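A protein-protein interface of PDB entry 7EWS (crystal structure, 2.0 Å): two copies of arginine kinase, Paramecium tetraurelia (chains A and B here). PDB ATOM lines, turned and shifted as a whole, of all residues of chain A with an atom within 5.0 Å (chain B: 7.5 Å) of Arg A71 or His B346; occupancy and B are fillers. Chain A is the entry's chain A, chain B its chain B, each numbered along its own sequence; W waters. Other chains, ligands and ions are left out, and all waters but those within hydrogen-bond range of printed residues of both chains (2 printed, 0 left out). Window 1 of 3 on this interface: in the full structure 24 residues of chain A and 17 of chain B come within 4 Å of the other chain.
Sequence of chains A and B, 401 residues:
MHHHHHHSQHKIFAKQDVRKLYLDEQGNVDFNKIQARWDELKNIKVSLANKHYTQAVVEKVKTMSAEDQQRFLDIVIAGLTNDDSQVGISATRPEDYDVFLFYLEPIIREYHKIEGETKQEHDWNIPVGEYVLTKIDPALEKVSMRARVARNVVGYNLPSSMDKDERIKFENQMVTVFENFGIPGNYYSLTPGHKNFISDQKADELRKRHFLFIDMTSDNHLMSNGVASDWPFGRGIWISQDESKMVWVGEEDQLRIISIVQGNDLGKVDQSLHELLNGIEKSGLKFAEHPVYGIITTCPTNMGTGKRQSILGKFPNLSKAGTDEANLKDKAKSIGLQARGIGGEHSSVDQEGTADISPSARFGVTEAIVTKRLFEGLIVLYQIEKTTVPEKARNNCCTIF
Arg A71 touches just one residue of chain B: His B346 (3.4 Å).
Of the printed residues of chain A, His B346 touches Arg A19 (3.8 Å), Gln A70 (3.2 Å), Arg A71 (3.4 Å), Asp A74 (2.4 Å) and Ser A161 (3.5 Å).
Printed residues of chain B within 4 Å of Glu A67: Glu B345.
Of the printed residues of chain B, Gln A70 touches His B346 and Ser B347.
Of the printed residues of chain B, Ser A161 touches His B346 (3.5 Å).
Of the printed residues of chain A, Ser B347 touches Gln A70 (3.7 Å).
Of the printed residues of chain A, Glu B345 touches Glu A67.
Gly B343 touches none of the printed residues of chain A.
Phe A100 touches none of the printed residues of chain B.
The nearest residue of chain B that does not touch Arg A71 is Glu B345 (6.6 Å).
The nearest printed residue of chain B that does not touch Glu A67 is His B346 (4.1 Å).
Water W1 lies within hydrogen-bond range of O of Glu B345 (2.6 Å), O of Gly B343 (2.7 Å) and N of Glu A67 (3.4 Å).
Water W2 lies within hydrogen-bond range of O of Gly B343 (2.6 Å) and NE2 of Gln A70 (3.0 Å).
No position is printed for both chains.
Of the 8 pairs that touch across the chains among the printed residues, none has its exchanged pair printed and touching as well.
The backbone carbonyl oxygen of Gly B341 sits close to the side-chain hydroxyl of Ser B347 (3.3 Å).
The guanidinium group (NH2) of Arg A19 lies within hydrogen-bond range of the side-chain amide oxygen (OE1) of Gln A70, at 2.9 Å.
OD1 of Asp A74 is in salt-bridge range of NE of Arg A19 (2.9 Å).
OE2 of Glu B345 is in salt-bridge range of NE of Arg B340 (2.5 Å).
The backbone carbonyl oxygen (O) of Gly B344 is in hydrogen-bond range of the side-chain hydroxyl (OG) of Ser B347.
The guanidinium group (NH2) of Arg A71 is in salt-bridge range of the side-chain carboxylate (OE2) of Glu A67 (3.1 Å).
Hydrophobic or aromatic side chains of chain B that line the printed part of chain A: His B346.
Among the printed residues, 8 pairs touch across the chains.
Among the printed residues, no Asp or Glu carboxylate lies within 4 Å of a Lys or Arg side-chain nitrogen of the other chain.
Among the printed residues, pairs that only touch across the chains: Arg A19 with His B346 (3.8 Å), Glu A67 with Glu B345 (3.6 Å), Gln A70 with His B346 (3.2 Å), Gln A70 with Ser B347 (3.7 Å), Arg A71 with His B346 (3.4 Å) and Ser A161 with His B346 (3.5 Å).
The side-chain hydroxyl (OG) of Ser B348 lies within hydrogen-bond range of the guanidinium group (NH1) of Arg A19, 2.9 Å away.
OD2 of Asp A74 sits close to NE2 of His B346 (2.4 Å).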
ATOM      1  N   ARG A  19      -2.030 -23.938   7.025  1.00  0.00           N
ATOM      2  CA  ARG A  19      -3.441 -23.513   7.276  1.00  0.00           C
ATOM      3  C   ARG A  19      -4.189 -23.460   5.940  1.00  0.00           C
ATOM      4  O   ARG A  19      -5.410 -23.672   5.908  1.00  0.00           O
ATOM      5  CB  ARG A  19      -3.545 -22.197   8.059  1.00  0.00           C
ATOM      6  CG  ARG A  19      -3.216 -20.930   7.282  1.00  0.00           C
ATOM      7  CD  ARG A  19      -3.155 -19.706   8.175  1.00  0.00           C
ATOM      8  NE  ARG A  19      -4.298 -19.643   9.076  1.00  0.00           N
ATOM      9  CZ  ARG A  19      -5.530 -19.337   8.708  1.00  0.00           C
ATOM     10  NH1 ARG A  19      -5.807 -18.975   7.461  1.00  0.00           N
ATOM     11  NH2 ARG A  19      -6.490 -19.329   9.611  1.00  0.00           N
ATOM     12  N   GLU A  67     -13.880 -14.417  11.324  1.00  0.00           N
ATOM     13  CA  GLU A  67     -12.575 -14.239  12.011  1.00  0.00           C
ATOM     14  C   GLU A  67     -12.398 -15.345  13.066  1.00  0.00           C
ATOM     15  O   GLU A  67     -11.304 -15.912  13.146  1.00  0.00           O
ATOM     16  CB  GLU A  67     -12.451 -12.847  12.643  1.00  0.00           C
ATOM     17  CG  GLU A  67     -11.101 -12.637  13.310  1.00  0.00           C
ATOM     18  CD  GLU A  67     -10.867 -11.279  13.950  1.00  0.00           C
ATOM     19  OE1 GLU A  67     -11.653 -10.361  13.684  1.00  0.00           O
ATOM     20  OE2 GLU A  67      -9.882 -11.142  14.704  1.00  0.00           O
ATOM     21  N   ASP A  68     -13.442 -15.637  13.832  1.00  0.00           N
ATOM     22  CA  ASP A  68     -13.453 -16.737  14.833  1.00  0.00           C
ATOM     23  C   ASP A  68     -13.288 -18.089  14.124  1.00  0.00           C
ATOM     24  O   ASP A  68     -12.623 -18.956  14.688  1.00  0.00           O
ATOM     25  CB  ASP A  68     -14.714 -16.733  15.692  1.00  0.00           C
ATOM     26  CG  ASP A  68     -14.727 -15.721  16.829  1.00  0.00           C
ATOM     27  OD1 ASP A  68     -13.628 -15.220  17.219  1.00  0.00           O
ATOM     28  OD2 ASP A  68     -15.853 -15.432  17.329  1.00  0.00           O
ATOM     29  N   GLN A  69     -13.838 -18.273  12.931  1.00  0.00           N
ATOM     30  CA  GLN A  69     -13.661 -19.560  12.212  1.00  0.00           C
ATOM     31  C   GLN A  69     -12.183 -19.756  11.864  1.00  0.00           C
ATOM     32  O   GLN A  69     -11.677 -20.851  12.045  1.00  0.00           O
ATOM     33  CB  GLN A  69     -14.505 -19.610  10.932  1.00  0.00           C
ATOM     34  CG  GLN A  69     -15.994 -19.666  11.208  1.00  0.00           C
ATOM     35  CD  GLN A  69     -16.818 -19.677   9.939  1.00  0.00           C
ATOM     36  OE1 GLN A  69     -16.304 -19.814   8.826  1.00  0.00           O
ATOM     37  NE2 GLN A  69     -18.106 -19.474  10.114  1.00  0.00           N
ATOM     38  N   GLN A  70     -11.541 -18.706  11.346  1.00  0.00           N
ATOM     39  CA  GLN A  70     -10.106 -18.697  10.974  1.00  0.00           C
ATOM     40  C   GLN A  70      -9.262 -18.978  12.222  1.00  0.00           C
ATOM     41  O   GLN A  70      -8.312 -19.747  12.144  1.00  0.00           O
ATOM     42  CB  GLN A  70      -9.741 -17.349  10.330  1.00  0.00           C
ATOM     43  CG  GLN A  70     -10.426 -17.096   8.986  1.00  0.00           C
ATOM     44  CD  GLN A  70      -9.772 -17.820   7.831  1.00  0.00           C
ATOM     45  OE1 GLN A  70      -8.688 -18.385   7.947  1.00  0.00           O
ATOM     46  NE2 GLN A  70     -10.437 -17.806   6.687  1.00  0.00           N
ATOM     47  N   ARG A  71      -9.616 -18.341  13.331  1.00  0.00           N
ATOM     48  CA  ARG A  71      -8.937 -18.530  14.636  1.00  0.00           C
ATOM     49  C   ARG A  71      -9.090 -20.000  15.070  1.00  0.00           C
ATOM     50  O   ARG A  71      -8.115 -20.625  15.522  1.00  0.00           O
ATOM     51  CB  ARG A  71      -9.509 -17.513  15.628  1.00  0.00           C
ATOM     52  CG  ARG A  71      -8.682 -17.373  16.896  1.00  0.00           C
ATOM     53  CD  ARG A  71      -9.067 -16.172  17.752  1.00  0.00           C
ATOM     54  NE  ARG A  71      -9.006 -14.909  17.050  1.00  0.00           N
ATOM     55  CZ  ARG A  71      -7.882 -14.268  16.719  1.00  0.00           C
ATOM     56  NH1 ARG A  71      -6.676 -14.750  17.022  1.00  0.00           N
ATOM     57  NH2 ARG A  71      -7.989 -13.111  16.093  1.00  0.00           N
ATOM     58  N   PHE A  72     -10.277 -20.560  14.888  1.00  0.00           N
ATOM     59  CA  PHE A  72     -10.567 -21.956  15.296  1.00  0.00           C
ATOM     60  C   PHE A  72      -9.615 -22.890  14.537  1.00  0.00           C
ATOM     61  O   PHE A  72      -9.006 -23.797  15.162  1.00  0.00           O
ATOM     62  CB  PHE A  72     -12.033 -22.282  15.037  1.00  0.00           C
ATOM     63  CG  PHE A  72     -12.369 -23.701  15.376  1.00  0.00           C
ATOM     64  CD1 PHE A  72     -12.692 -24.046  16.671  1.00  0.00           C
ATOM     65  CD2 PHE A  72     -12.295 -24.690  14.416  1.00  0.00           C
ATOM     66  CE1 PHE A  72     -12.930 -25.359  17.016  1.00  0.00           C
ATOM     67  CE2 PHE A  72     -12.544 -26.013  14.772  1.00  0.00           C
ATOM     68  CZ  PHE A  72     -12.882 -26.338  16.062  1.00  0.00           C
ATOM     69  N   LEU A  73      -9.468 -22.664  13.224  1.00  0.00           N
ATOM     70  CA  LEU A  73      -8.497 -23.415  12.379  1.00  0.00           C
ATOM     71  C   LEU A  73      -7.077 -23.280  12.977  1.00  0.00           C
ATOM     72  O   LEU A  73      -6.409 -24.326  13.136  1.00  0.00           O
ATOM     73  CB  LEU A  73      -8.557 -22.953  10.917  1.00  0.00           C
ATOM     74  CG  LEU A  73      -7.456 -23.530  10.037  1.00  0.00           C
ATOM     75  CD1 LEU A  73      -7.485 -25.058  10.055  1.00  0.00           C
ATOM     76  CD2 LEU A  73      -7.515 -22.979   8.608  1.00  0.00           C
ATOM     77  N   ASP A  74      -6.660 -22.078  13.391  1.00  0.00           N
ATOM     78  CA  ASP A  74      -5.328 -21.882  14.009  1.00  0.00           C
ATOM     79  C   ASP A  74      -5.229 -22.630  15.337  1.00  0.00           C
ATOM     80  O   ASP A  74      -4.111 -22.953  15.710  1.00  0.00           O
ATOM     81  CB  ASP A  74      -4.994 -20.400  14.173  1.00  0.00           C
ATOM     82  CG  ASP A  74      -4.618 -19.736  12.848  1.00  0.00           C
ATOM     83  OD1 ASP A  74      -4.543 -20.461  11.809  1.00  0.00           O
ATOM     84  OD2 ASP A  74      -4.444 -18.504  12.855  1.00  0.00           O
ATOM     85  N   ILE A  75      -6.332 -22.850  16.042  1.00  0.00           N
ATOM     86  CA  ILE A  75      -6.309 -23.556  17.355  1.00  0.00           C
ATOM     87  C   ILE A  75      -6.097 -25.060  17.148  1.00  0.00           C
ATOM     88  O   ILE A  75      -5.455 -25.662  17.995  1.00  0.00           O
ATOM     89  CB  ILE A  75      -7.573 -23.242  18.184  1.00  0.00           C
ATOM     90  CG1 ILE A  75      -7.519 -21.797  18.679  1.00  0.00           C
ATOM     91  CG2 ILE A  75      -7.734 -24.233  19.335  1.00  0.00           C
ATOM     92  CD1 ILE A  75      -8.852 -21.251  19.054  1.00  0.00           C
ATOM     93  N   THR A  92      -4.603 -18.937  20.698  1.00  0.00           N
ATOM     94  CA  THR A  92      -3.950 -17.804  19.977  1.00  0.00           C
ATOM     95  C   THR A  92      -3.964 -16.517  20.813  1.00  0.00           C
ATOM     96  O   THR A  92      -3.145 -15.611  20.543  1.00  0.00           O
ATOM     97  CB  THR A  92      -4.549 -17.607  18.580  1.00  0.00           C
ATOM     98  OG1 THR A  92      -5.829 -17.008  18.671  1.00  0.00           O
ATOM     99  CG2 THR A  92      -4.647 -18.907  17.806  1.00  0.00           C
ATOM    100  N   ARG A  93      -4.872 -16.428  21.778  1.00  0.00           N
ATOM    101  CA  ARG A  93      -5.061 -15.243  22.636  1.00  0.00           C
ATOM    102  C   ARG A  93      -5.548 -15.719  23.997  1.00  0.00           C
ATOM    103  O   ARG A  93      -6.220 -16.751  24.065  1.00  0.00           O
ATOM    104  CB  ARG A  93      -6.117 -14.288  22.063  1.00  0.00           C
ATOM    105  CG  ARG A  93      -5.957 -13.891  20.602  1.00  0.00           C
ATOM    106  CD  ARG A  93      -7.192 -13.157  20.092  1.00  0.00           C
ATOM    107  NE  ARG A  93      -8.368 -14.003  20.189  1.00  0.00           N
ATOM    108  CZ  ARG A  93      -9.620 -13.634  19.913  1.00  0.00           C
ATOM    109  NH1 ARG A  93      -9.874 -12.416  19.463  1.00  0.00           N
ATOM    110  NH2 ARG A  93     -10.603 -14.516  20.071  1.00  0.00           N
ATOM    111  N   ASP A  96      -9.184 -16.825  24.147  1.00  0.00           N
ATOM    112  CA  ASP A  96      -9.617 -18.005  23.352  1.00  0.00           C
ATOM    113  C   ASP A  96     -10.220 -19.102  24.250  1.00  0.00           C
ATOM    114  O   ASP A  96     -11.095 -19.841  23.748  1.00  0.00           O
ATOM    115  CB  ASP A  96      -8.502 -18.596  22.510  1.00  0.00           C
ATOM    116  CG  ASP A  96      -8.192 -17.799  21.267  1.00  0.00           C
ATOM    117  OD1 ASP A  96      -8.859 -16.764  21.033  1.00  0.00           O
ATOM    118  OD2 ASP A  96      -7.252 -18.203  20.574  1.00  0.00           O
ATOM    119  N   PHE A 100     -13.866 -20.158  22.887  1.00  0.00           N
ATOM    120  CA  PHE A 100     -13.987 -21.520  22.304  1.00  0.00           C
ATOM    121  C   PHE A 100     -14.145 -22.566  23.409  1.00  0.00           C
ATOM    122  O   PHE A 100     -13.817 -23.749  23.193  1.00  0.00           O
ATOM    123  CB  PHE A 100     -12.788 -21.821  21.417  1.00  0.00           C
ATOM    124  CG  PHE A 100     -12.652 -20.872  20.256  1.00  0.00           C
ATOM    125  CD1 PHE A 100     -13.486 -21.010  19.152  1.00  0.00           C
ATOM    126  CD2 PHE A 100     -11.715 -19.849  20.260  1.00  0.00           C
ATOM    127  CE1 PHE A 100     -13.385 -20.156  18.067  1.00  0.00           C
ATOM    128  CE2 PHE A 100     -11.597 -19.008  19.161  1.00  0.00           C
ATOM    129  CZ  PHE A 100     -12.420 -19.167  18.066  1.00  0.00           C
ATOM    130  N   SER A 161       0.516 -16.696  17.927  1.00  0.00           N
ATOM    131  CA  SER A 161      -0.136 -15.700  17.040  1.00  0.00           C
ATOM    132  C   SER A 161       0.470 -14.302  17.199  1.00  0.00           C
ATOM    133  O   SER A 161      -0.304 -13.331  17.116  1.00  0.00           O
ATOM    134  CB  SER A 161      -1.614 -15.647  17.303  1.00  0.00           C
ATOM    135  OG  SER A 161      -2.320 -15.251  16.133  1.00  0.00           O
ATOM    136  N   GLU B 325       3.440 -13.315   3.307  1.00  0.00           N
ATOM    137  CA  GLU B 325       2.364 -12.318   3.505  1.00  0.00           C
ATOM    138  C   GLU B 325       2.950 -11.079   4.206  1.00  0.00           C
ATOM    139  O   GLU B 325       2.547  -9.948   3.857  1.00  0.00           O
ATOM    140  CB  GLU B 325       1.223 -12.973   4.284  1.00  0.00           C
ATOM    141  CG  GLU B 325       0.603 -14.151   3.557  1.00  0.00           C
ATOM    142  CD  GLU B 325      -0.532 -14.834   4.314  1.00  0.00           C
ATOM    143  OE1 GLU B 325      -0.751 -14.470   5.481  1.00  0.00           O
ATOM    144  OE2 GLU B 325      -1.178 -15.728   3.742  1.00  0.00           O
ATOM    145  N   LYS B 329       2.388  -7.136   3.334  1.00  0.00           N
ATOM    146  CA  LYS B 329       1.758  -6.231   4.342  1.00  0.00           C
ATOM    147  C   LYS B 329       2.721  -5.083   4.657  1.00  0.00           C
ATOM    148  O   LYS B 329       2.260  -3.943   4.745  1.00  0.00           O
ATOM    149  CB  LYS B 329       1.339  -6.987   5.610  1.00  0.00           C
ATOM    150  CG  LYS B 329       0.350  -8.111   5.340  1.00  0.00           C
ATOM    151  CD  LYS B 329      -0.239  -8.797   6.552  1.00  0.00           C
ATOM    152  CE  LYS B 329      -1.010 -10.015   6.076  1.00  0.00           C
ATOM    153  NZ  LYS B 329      -1.721 -10.693   7.172  1.00  0.00           N
ATOM    154  N   ARG B 340      -4.577  -7.737   3.513  1.00  0.00           N
ATOM    155  CA  ARG B 340      -5.088  -8.847   4.352  1.00  0.00           C
ATOM    156  C   ARG B 340      -5.389 -10.026   3.433  1.00  0.00           C
ATOM    157  O   ARG B 340      -5.452  -9.823   2.186  1.00  0.00           O
ATOM    158  CB  ARG B 340      -6.366  -8.433   5.097  1.00  0.00           C
ATOM    159  CG  ARG B 340      -6.197  -7.274   6.076  1.00  0.00           C
ATOM    160  CD  ARG B 340      -7.557  -6.948   6.659  1.00  0.00           C
ATOM    161  NE  ARG B 340      -7.638  -6.073   7.825  1.00  0.00           N
ATOM    162  CZ  ARG B 340      -6.623  -5.626   8.575  1.00  0.00           C
ATOM    163  NH1 ARG B 340      -5.370  -5.935   8.298  1.00  0.00           N
ATOM    164  NH2 ARG B 340      -6.884  -4.845   9.609  1.00  0.00           N
ATOM    165  N   GLY B 341      -5.634 -11.194   4.029  1.00  0.00           N
ATOM    166  CA  GLY B 341      -6.055 -12.378   3.267  1.00  0.00           C
ATOM    167  C   GLY B 341      -7.412 -12.144   2.619  1.00  0.00           C
ATOM    168  O   GLY B 341      -8.082 -11.158   2.957  1.00  0.00           O
ATOM    169  N   GLY B 343     -10.113 -13.904   3.038  1.00  0.00           N
ATOM    170  CA  GLY B 343     -11.238 -14.360   3.884  1.00  0.00           C
ATOM    171  C   GLY B 343     -11.459 -13.484   5.108  1.00  0.00           C
ATOM    172  O   GLY B 343     -11.956 -14.009   6.132  1.00  0.00           O
ATOM    173  N   GLY B 344     -11.059 -12.213   5.050  1.00  0.00           N
ATOM    174  CA  GLY B 344     -11.298 -11.236   6.134  1.00  0.00           C
ATOM    175  C   GLY B 344     -10.103 -11.147   7.068  1.00  0.00           C
ATOM    176  O   GLY B 344      -8.979 -11.577   6.681  1.00  0.00           O
ATOM    177  N   GLU B 345     -10.310 -10.594   8.258  1.00  0.00           N
ATOM    178  CA  GLU B 345      -9.265 -10.532   9.307  1.00  0.00           C
ATOM    179  C   GLU B 345      -8.805 -11.958   9.621  1.00  0.00           C
ATOM    180  O   GLU B 345      -9.682 -12.850   9.675  1.00  0.00           O
ATOM    181  CB  GLU B 345      -9.810  -9.908  10.591  1.00  0.00           C
ATOM    182  CG  GLU B 345     -10.251  -8.478  10.430  1.00  0.00           C
ATOM    183  CD  GLU B 345      -9.132  -7.529  10.042  1.00  0.00           C
ATOM    184  OE1 GLU B 345      -7.946  -7.867  10.273  1.00  0.00           O
ATOM    185  OE2 GLU B 345      -9.457  -6.435   9.501  1.00  0.00           O
ATOM    186  N   HIS B 346      -7.503 -12.141   9.843  1.00  0.00           N
ATOM    187  CA  HIS B 346      -6.891 -13.390  10.370  1.00  0.00           C
ATOM    188  C   HIS B 346      -7.064 -14.470   9.311  1.00  0.00           C
ATOM    189  O   HIS B 346      -7.171 -15.633   9.687  1.00  0.00           O
ATOM    190  CB  HIS B 346      -7.510 -13.812  11.724  1.00  0.00           C
ATOM    191  CG  HIS B 346      -6.655 -14.757  12.521  1.00  0.00           C
ATOM    192  ND1 HIS B 346      -5.773 -14.322  13.519  1.00  0.00           N
ATOM    193  CD2 HIS B 346      -6.512 -16.105  12.464  1.00  0.00           C
ATOM    194  CE1 HIS B 346      -5.129 -15.348  14.038  1.00  0.00           C
ATOM    195  NE2 HIS B 346      -5.565 -16.461  13.397  1.00  0.00           N
ATOM    196  N   SER B 347      -7.062 -14.113   8.030  1.00  0.00           N
ATOM    197  CA  SER B 347      -7.200 -15.078   6.907  1.00  0.00           C
ATOM    198  C   SER B 347      -5.883 -15.162   6.118  1.00  0.00           C
ATOM    199  O   SER B 347      -4.878 -14.689   6.607  1.00  0.00           O
ATOM    200  CB  SER B 347      -8.382 -14.740   6.042  1.00  0.00           C
ATOM    201  OG  SER B 347      -8.130 -13.578   5.253  1.00  0.00           O
ATOM    202  N   SER B 348      -5.864 -15.795   4.954  1.00  0.00           N
ATOM    203  CA  SER B 348      -4.609 -16.082   4.202  1.00  0.00           C
ATOM    204  C   SER B 348      -4.602 -15.409   2.823  1.00  0.00           C
ATOM    205  O   SER B 348      -5.631 -15.363   2.121  1.00  0.00           O
ATOM    206  CB  SER B 348      -4.367 -17.570   4.064  1.00  0.00           C
ATOM    207  OG  SER B 348      -4.072 -18.157   5.321  1.00  0.00           O
HETATM  208  O   HOH W   1     -12.078 -13.281   8.723  1.00  0.00           O
HETATM  209  O   HOH W   2     -13.009 -16.417   6.188  1.00  0.00           O
